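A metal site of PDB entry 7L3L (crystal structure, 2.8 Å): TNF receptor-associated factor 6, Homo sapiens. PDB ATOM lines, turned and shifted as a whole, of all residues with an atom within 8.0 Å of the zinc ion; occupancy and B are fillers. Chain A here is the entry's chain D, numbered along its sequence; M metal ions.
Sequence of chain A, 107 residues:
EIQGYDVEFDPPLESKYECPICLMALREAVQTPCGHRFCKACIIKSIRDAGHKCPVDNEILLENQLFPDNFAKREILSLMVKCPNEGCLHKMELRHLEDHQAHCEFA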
ATOM      1  N   GLN A   3     -15.380   2.748 -25.274  1.00  0.00           N
ATOM      2  CA  GLN A   3     -16.772   2.905 -24.883  1.00  0.00           C
ATOM      3  C   GLN A   3     -17.340   4.261 -25.298  1.00  0.00           C
ATOM      4  O   GLN A   3     -17.705   5.074 -24.455  1.00  0.00           O
ATOM      5  CB  GLN A   3     -16.922   2.727 -23.368  1.00  0.00           C
ATOM      6  CG  GLN A   3     -16.635   1.311 -22.884  1.00  0.00           C
ATOM      7  CD  GLN A   3     -15.339   1.219 -22.107  1.00  0.00           C
ATOM      8  OE1 GLN A   3     -14.826   2.218 -21.613  1.00  0.00           O
ATOM      9  NE2 GLN A   3     -14.797   0.003 -21.993  1.00  0.00           N
ATOM     10  N   GLY A   4     -17.409   4.499 -26.608  1.00  0.00           N
ATOM     11  CA  GLY A   4     -18.063   5.673 -27.140  1.00  0.00           C
ATOM     12  C   GLY A   4     -19.571   5.533 -27.114  1.00  0.00           C
ATOM     13  O   GLY A   4     -20.130   4.739 -26.345  1.00  0.00           O
ATOM     14  N   TYR A   5     -20.239   6.304 -27.954  1.00  0.00           N
ATOM     15  CA  TYR A   5     -21.702   6.313 -28.025  1.00  0.00           C
ATOM     16  C   TYR A   5     -22.168   5.479 -29.222  1.00  0.00           C
ATOM     17  O   TYR A   5     -21.900   5.822 -30.378  1.00  0.00           O
ATOM     18  CB  TYR A   5     -22.237   7.737 -28.135  1.00  0.00           C
ATOM     19  CG  TYR A   5     -22.096   8.540 -26.865  1.00  0.00           C
ATOM     20  CD1 TYR A   5     -22.675   8.104 -25.681  1.00  0.00           C
ATOM     21  CD2 TYR A   5     -21.392   9.735 -26.851  1.00  0.00           C
ATOM     22  CE1 TYR A   5     -22.551   8.837 -24.509  1.00  0.00           C
ATOM     23  CE2 TYR A   5     -21.263  10.474 -25.685  1.00  0.00           C
ATOM     24  CZ  TYR A   5     -21.839  10.016 -24.519  1.00  0.00           C
ATOM     25  OH  TYR A   5     -21.715  10.751 -23.360  1.00  0.00           O
ATOM     26  N   GLU A  18     -15.857  11.968 -34.092  1.00  0.00           N
ATOM     27  CA  GLU A  18     -15.717  10.524 -34.060  1.00  0.00           C
ATOM     28  C   GLU A  18     -14.392  10.153 -33.420  1.00  0.00           C
ATOM     29  O   GLU A  18     -13.349  10.750 -33.729  1.00  0.00           O
ATOM     30  CB  GLU A  18     -15.806   9.949 -35.479  1.00  0.00           C
ATOM     31  CG  GLU A  18     -15.540   8.462 -35.586  1.00  0.00           C
ATOM     32  CD  GLU A  18     -15.648   7.968 -37.028  1.00  0.00           C
ATOM     33  OE1 GLU A  18     -16.290   6.923 -37.239  1.00  0.00           O
ATOM     34  OE2 GLU A  18     -15.093   8.627 -37.927  1.00  0.00           O
ATOM     35  N   CYS A  19     -14.424   9.166 -32.525  1.00  0.00           N
ATOM     36  CA  CYS A  19     -13.212   8.750 -31.815  1.00  0.00           C
ATOM     37  C   CYS A  19     -12.402   7.798 -32.669  1.00  0.00           C
ATOM     38  O   CYS A  19     -12.901   6.727 -33.038  1.00  0.00           O
ATOM     39  CB  CYS A  19     -13.580   8.080 -30.499  1.00  0.00           C
ATOM     40  SG  CYS A  19     -12.198   7.227 -29.718  1.00  0.00           S
ATOM     41  N   PRO A  20     -11.156   8.123 -33.002  1.00  0.00           N
ATOM     42  CA  PRO A  20     -10.388   7.276 -33.926  1.00  0.00           C
ATOM     43  C   PRO A  20     -10.128   5.873 -33.405  1.00  0.00           C
ATOM     44  O   PRO A  20      -9.854   4.974 -34.214  1.00  0.00           O
ATOM     45  CB  PRO A  20      -9.073   8.049 -34.122  1.00  0.00           C
ATOM     46  CG  PRO A  20      -9.362   9.439 -33.650  1.00  0.00           C
ATOM     47  CD  PRO A  20     -10.380   9.297 -32.567  1.00  0.00           C
ATOM     48  N   ILE A  21     -10.189   5.653 -32.095  1.00  0.00           N
ATOM     49  CA  ILE A  21      -9.859   4.348 -31.535  1.00  0.00           C
ATOM     50  C   ILE A  21     -11.074   3.429 -31.582  1.00  0.00           C
ATOM     51  O   ILE A  21     -11.010   2.337 -32.155  1.00  0.00           O
ATOM     52  CB  ILE A  21      -9.316   4.464 -30.106  1.00  0.00           C
ATOM     53  CG1 ILE A  21      -7.999   5.250 -30.092  1.00  0.00           C
ATOM     54  CG2 ILE A  21      -9.132   3.086 -29.482  1.00  0.00           C
ATOM     55  CD1 ILE A  21      -7.108   4.998 -31.298  1.00  0.00           C
ATOM     56  N   CYS A  22     -12.184   3.865 -30.990  1.00  0.00           N
ATOM     57  CA  CYS A  22     -13.403   3.064 -30.947  1.00  0.00           C
ATOM     58  C   CYS A  22     -14.311   3.278 -32.146  1.00  0.00           C
ATOM     59  O   CYS A  22     -15.229   2.486 -32.366  1.00  0.00           O
ATOM     60  CB  CYS A  22     -14.180   3.353 -29.653  1.00  0.00           C
ATOM     61  SG  CYS A  22     -14.947   4.976 -29.572  1.00  0.00           S
ATOM     62  N   LEU A  23     -14.070   4.331 -32.939  1.00  0.00           N
ATOM     63  CA  LEU A  23     -14.841   4.629 -34.151  1.00  0.00           C
ATOM     64  C   LEU A  23     -16.309   4.933 -33.853  1.00  0.00           C
ATOM     65  O   LEU A  23     -17.192   4.714 -34.683  1.00  0.00           O
ATOM     66  CB  LEU A  23     -14.730   3.493 -35.180  1.00  0.00           C
ATOM     67  CG  LEU A  23     -13.332   3.371 -35.795  1.00  0.00           C
ATOM     68  CD1 LEU A  23     -13.315   2.335 -36.897  1.00  0.00           C
ATOM     69  CD2 LEU A  23     -12.872   4.731 -36.319  1.00  0.00           C
ATOM     70  N   MET A  24     -16.582   5.443 -32.654  1.00  0.00           N
ATOM     71  CA  MET A  24     -17.906   5.890 -32.258  1.00  0.00           C
ATOM     72  C   MET A  24     -17.795   7.302 -31.688  1.00  0.00           C
ATOM     73  O   MET A  24     -16.690   7.817 -31.478  1.00  0.00           O
ATOM     74  CB  MET A  24     -18.544   4.925 -31.246  1.00  0.00           C
ATOM     75  CG  MET A  24     -18.040   3.504 -31.373  1.00  0.00           C
ATOM     76  SD  MET A  24     -19.094   2.276 -30.570  1.00  0.00           S
ATOM     77  CE  MET A  24     -18.866   2.677 -28.846  1.00  0.00           C
ATOM     78  N   ALA A  25     -18.951   7.921 -31.454  1.00  0.00           N
ATOM     79  CA  ALA A  25     -18.965   9.263 -30.897  1.00  0.00           C
ATOM     80  C   ALA A  25     -18.166   9.329 -29.599  1.00  0.00           C
ATOM     81  O   ALA A  25     -18.208   8.410 -28.779  1.00  0.00           O
ATOM     82  CB  ALA A  25     -20.401   9.724 -30.652  1.00  0.00           C
ATOM     83  N   LEU A  26     -17.422  10.418 -29.436  1.00  0.00           N
ATOM     84  CA  LEU A  26     -16.568  10.565 -28.274  1.00  0.00           C
ATOM     85  C   LEU A  26     -17.394  10.609 -26.991  1.00  0.00           C
ATOM     86  O   LEU A  26     -18.406  11.311 -26.913  1.00  0.00           O
ATOM     87  CB  LEU A  26     -15.727  11.834 -28.395  1.00  0.00           C
ATOM     88  CG  LEU A  26     -15.002  12.044 -29.726  1.00  0.00           C
ATOM     89  CD1 LEU A  26     -14.956  13.512 -30.093  1.00  0.00           C
ATOM     90  CD2 LEU A  26     -13.611  11.496 -29.635  1.00  0.00           C
ATOM     91  N   ARG A  27     -16.960   9.849 -25.991  1.00  0.00           N
ATOM     92  CA  ARG A  27     -17.564   9.870 -24.664  1.00  0.00           C
ATOM     93  C   ARG A  27     -16.550  10.441 -23.681  1.00  0.00           C
ATOM     94  O   ARG A  27     -15.415   9.949 -23.602  1.00  0.00           O
ATOM     95  CB  ARG A  27     -17.993   8.480 -24.222  1.00  0.00           C
ATOM     96  CG  ARG A  27     -18.872   8.496 -22.981  1.00  0.00           C
ATOM     97  CD  ARG A  27     -18.818   7.187 -22.228  1.00  0.00           C
ATOM     98  NE  ARG A  27     -19.264   6.078 -23.060  1.00  0.00           N
ATOM     99  CZ  ARG A  27     -20.534   5.730 -23.211  1.00  0.00           C
ATOM    100  NH1 ARG A  27     -21.487   6.412 -22.590  1.00  0.00           N
ATOM    101  NH2 ARG A  27     -20.847   4.707 -23.990  1.00  0.00           N
ATOM    102  N   ARG A  37      -9.056  14.468 -31.025  1.00  0.00           N
ATOM    103  CA  ARG A  37      -9.997  14.154 -29.953  1.00  0.00           C
ATOM    104  C   ARG A  37     -10.133  12.637 -29.810  1.00  0.00           C
ATOM    105  O   ARG A  37     -10.137  11.906 -30.807  1.00  0.00           O
ATOM    106  CB  ARG A  37     -11.370  14.772 -30.240  1.00  0.00           C
ATOM    107  CG  ARG A  37     -11.316  16.191 -30.794  1.00  0.00           C
ATOM    108  CD  ARG A  37     -12.679  16.868 -30.757  1.00  0.00           C
ATOM    109  NE  ARG A  37     -13.067  17.425 -32.053  1.00  0.00           N
ATOM    110  CZ  ARG A  37     -13.118  18.725 -32.320  1.00  0.00           C
ATOM    111  NH1 ARG A  37     -12.815  19.611 -31.384  1.00  0.00           N
ATOM    112  NH2 ARG A  37     -13.477  19.136 -33.532  1.00  0.00           N
ATOM    113  N   PHE A  38     -10.231  12.190 -28.566  1.00  0.00           N
ATOM    114  CA  PHE A  38     -10.530  10.811 -28.227  1.00  0.00           C
ATOM    115  C   PHE A  38     -11.501  10.793 -27.051  1.00  0.00           C
ATOM    116  O   PHE A  38     -11.660  11.795 -26.337  1.00  0.00           O
ATOM    117  CB  PHE A  38      -9.265  10.016 -27.841  1.00  0.00           C
ATOM    118  CG  PHE A  38      -8.188  10.031 -28.893  1.00  0.00           C
ATOM    119  CD1 PHE A  38      -7.224  11.031 -28.911  1.00  0.00           C
ATOM    120  CD2 PHE A  38      -8.124   9.032 -29.852  1.00  0.00           C
ATOM    121  CE1 PHE A  38      -6.226  11.043 -29.872  1.00  0.00           C
ATOM    122  CE2 PHE A  38      -7.132   9.038 -30.808  1.00  0.00           C
ATOM    123  CZ  PHE A  38      -6.191  10.044 -30.825  1.00  0.00           C
ATOM    124  N   CYS A  39     -12.186   9.671 -26.881  1.00  0.00           N
ATOM    125  CA  CYS A  39     -12.803   9.388 -25.588  1.00  0.00           C
ATOM    126  C   CYS A  39     -11.718   9.363 -24.512  1.00  0.00           C
ATOM    127  O   CYS A  39     -10.566   9.013 -24.774  1.00  0.00           O
ATOM    128  CB  CYS A  39     -13.532   8.048 -25.597  1.00  0.00           C
ATOM    129  SG  CYS A  39     -14.927   7.901 -26.751  1.00  0.00           S
ATOM    130  N   LYS A  40     -12.088   9.742 -23.293  1.00  0.00           N
ATOM    131  CA  LYS A  40     -11.140   9.631 -22.191  1.00  0.00           C
ATOM    132  C   LYS A  40     -10.698   8.183 -22.023  1.00  0.00           C
ATOM    133  O   LYS A  40      -9.498   7.895 -21.924  1.00  0.00           O
ATOM    134  CB  LYS A  40     -11.745  10.169 -20.904  1.00  0.00           C
ATOM    135  CG  LYS A  40     -10.724  10.733 -19.922  1.00  0.00           C
ATOM    136  CD  LYS A  40     -11.393  11.430 -18.739  1.00  0.00           C
ATOM    137  CE  LYS A  40     -11.906  10.427 -17.715  1.00  0.00           C
ATOM    138  NZ  LYS A  40     -12.313  11.089 -16.446  1.00  0.00           N
ATOM    139  N   ALA A  41     -11.650   7.252 -22.045  1.00  0.00           N
ATOM    140  CA  ALA A  41     -11.351   5.852 -21.780  1.00  0.00           C
ATOM    141  C   ALA A  41     -10.431   5.269 -22.845  1.00  0.00           C
ATOM    142  O   ALA A  41      -9.447   4.584 -22.542  1.00  0.00           O
ATOM    143  CB  ALA A  41     -12.646   5.043 -21.683  1.00  0.00           C
ATOM    144  N   CYS A  42     -10.721   5.547 -24.118  1.00  0.00           N
ATOM    145  CA  CYS A  42     -10.034   4.867 -25.205  1.00  0.00           C
ATOM    146  C   CYS A  42      -8.570   5.302 -25.321  1.00  0.00           C
ATOM    147  O   CYS A  42      -7.704   4.491 -25.650  1.00  0.00           O
ATOM    148  CB  CYS A  42     -10.764   5.095 -26.526  1.00  0.00           C
ATOM    149  SG  CYS A  42     -12.365   4.282 -26.624  1.00  0.00           S
ATOM    150  N   ILE A  43      -8.281   6.575 -25.033  1.00  0.00           N
ATOM    151  CA  ILE A  43      -6.905   7.032 -25.190  1.00  0.00           C
ATOM    152  C   ILE A  43      -6.052   6.673 -23.980  1.00  0.00           C
ATOM    153  O   ILE A  43      -4.869   6.361 -24.114  1.00  0.00           O
ATOM    154  CB  ILE A  43      -6.860   8.542 -25.487  1.00  0.00           C
ATOM    155  CG1 ILE A  43      -5.430   8.987 -25.788  1.00  0.00           C
ATOM    156  CG2 ILE A  43      -7.436   9.353 -24.327  1.00  0.00           C
ATOM    157  CD1 ILE A  43      -4.748   8.182 -26.880  1.00  0.00           C
HETATM  158 ZN    ZN M   1     -13.530   6.180 -28.013  1.00  0.00          ZN
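The zinc ion is bound by SG of Cys 19 (2.4 Å), SG of Cys 22 (2.4 Å), SG of Cys 39 (2.6 Å) and SG of Cys 42 (2.6 Å). The zinc ion has four donor atoms within binding distance.
Four residues have an atom within 4 Å of the zinc ion: Cys 19, Cys 22, Cys 39 and Cys 42. The nearest printed residue that does not touch the zinc ion is Gly 4 (4.5 Å).
N of Cys 19 sits at hydrogen-bond distance from O of Met 24, 2.8 Å away. The side-chain sulfur of Cys 19 sits close to the backbone NH of Ile 21, at 3.5 Å. SG of Cys 22 lies close to N of Met 24 (3.5 Å). SG of Cys 39 lies close to N of Arg 27, at 2.9 Å. N of Gln 3 lies close to SG of Cys 42, at 3.6 Å.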
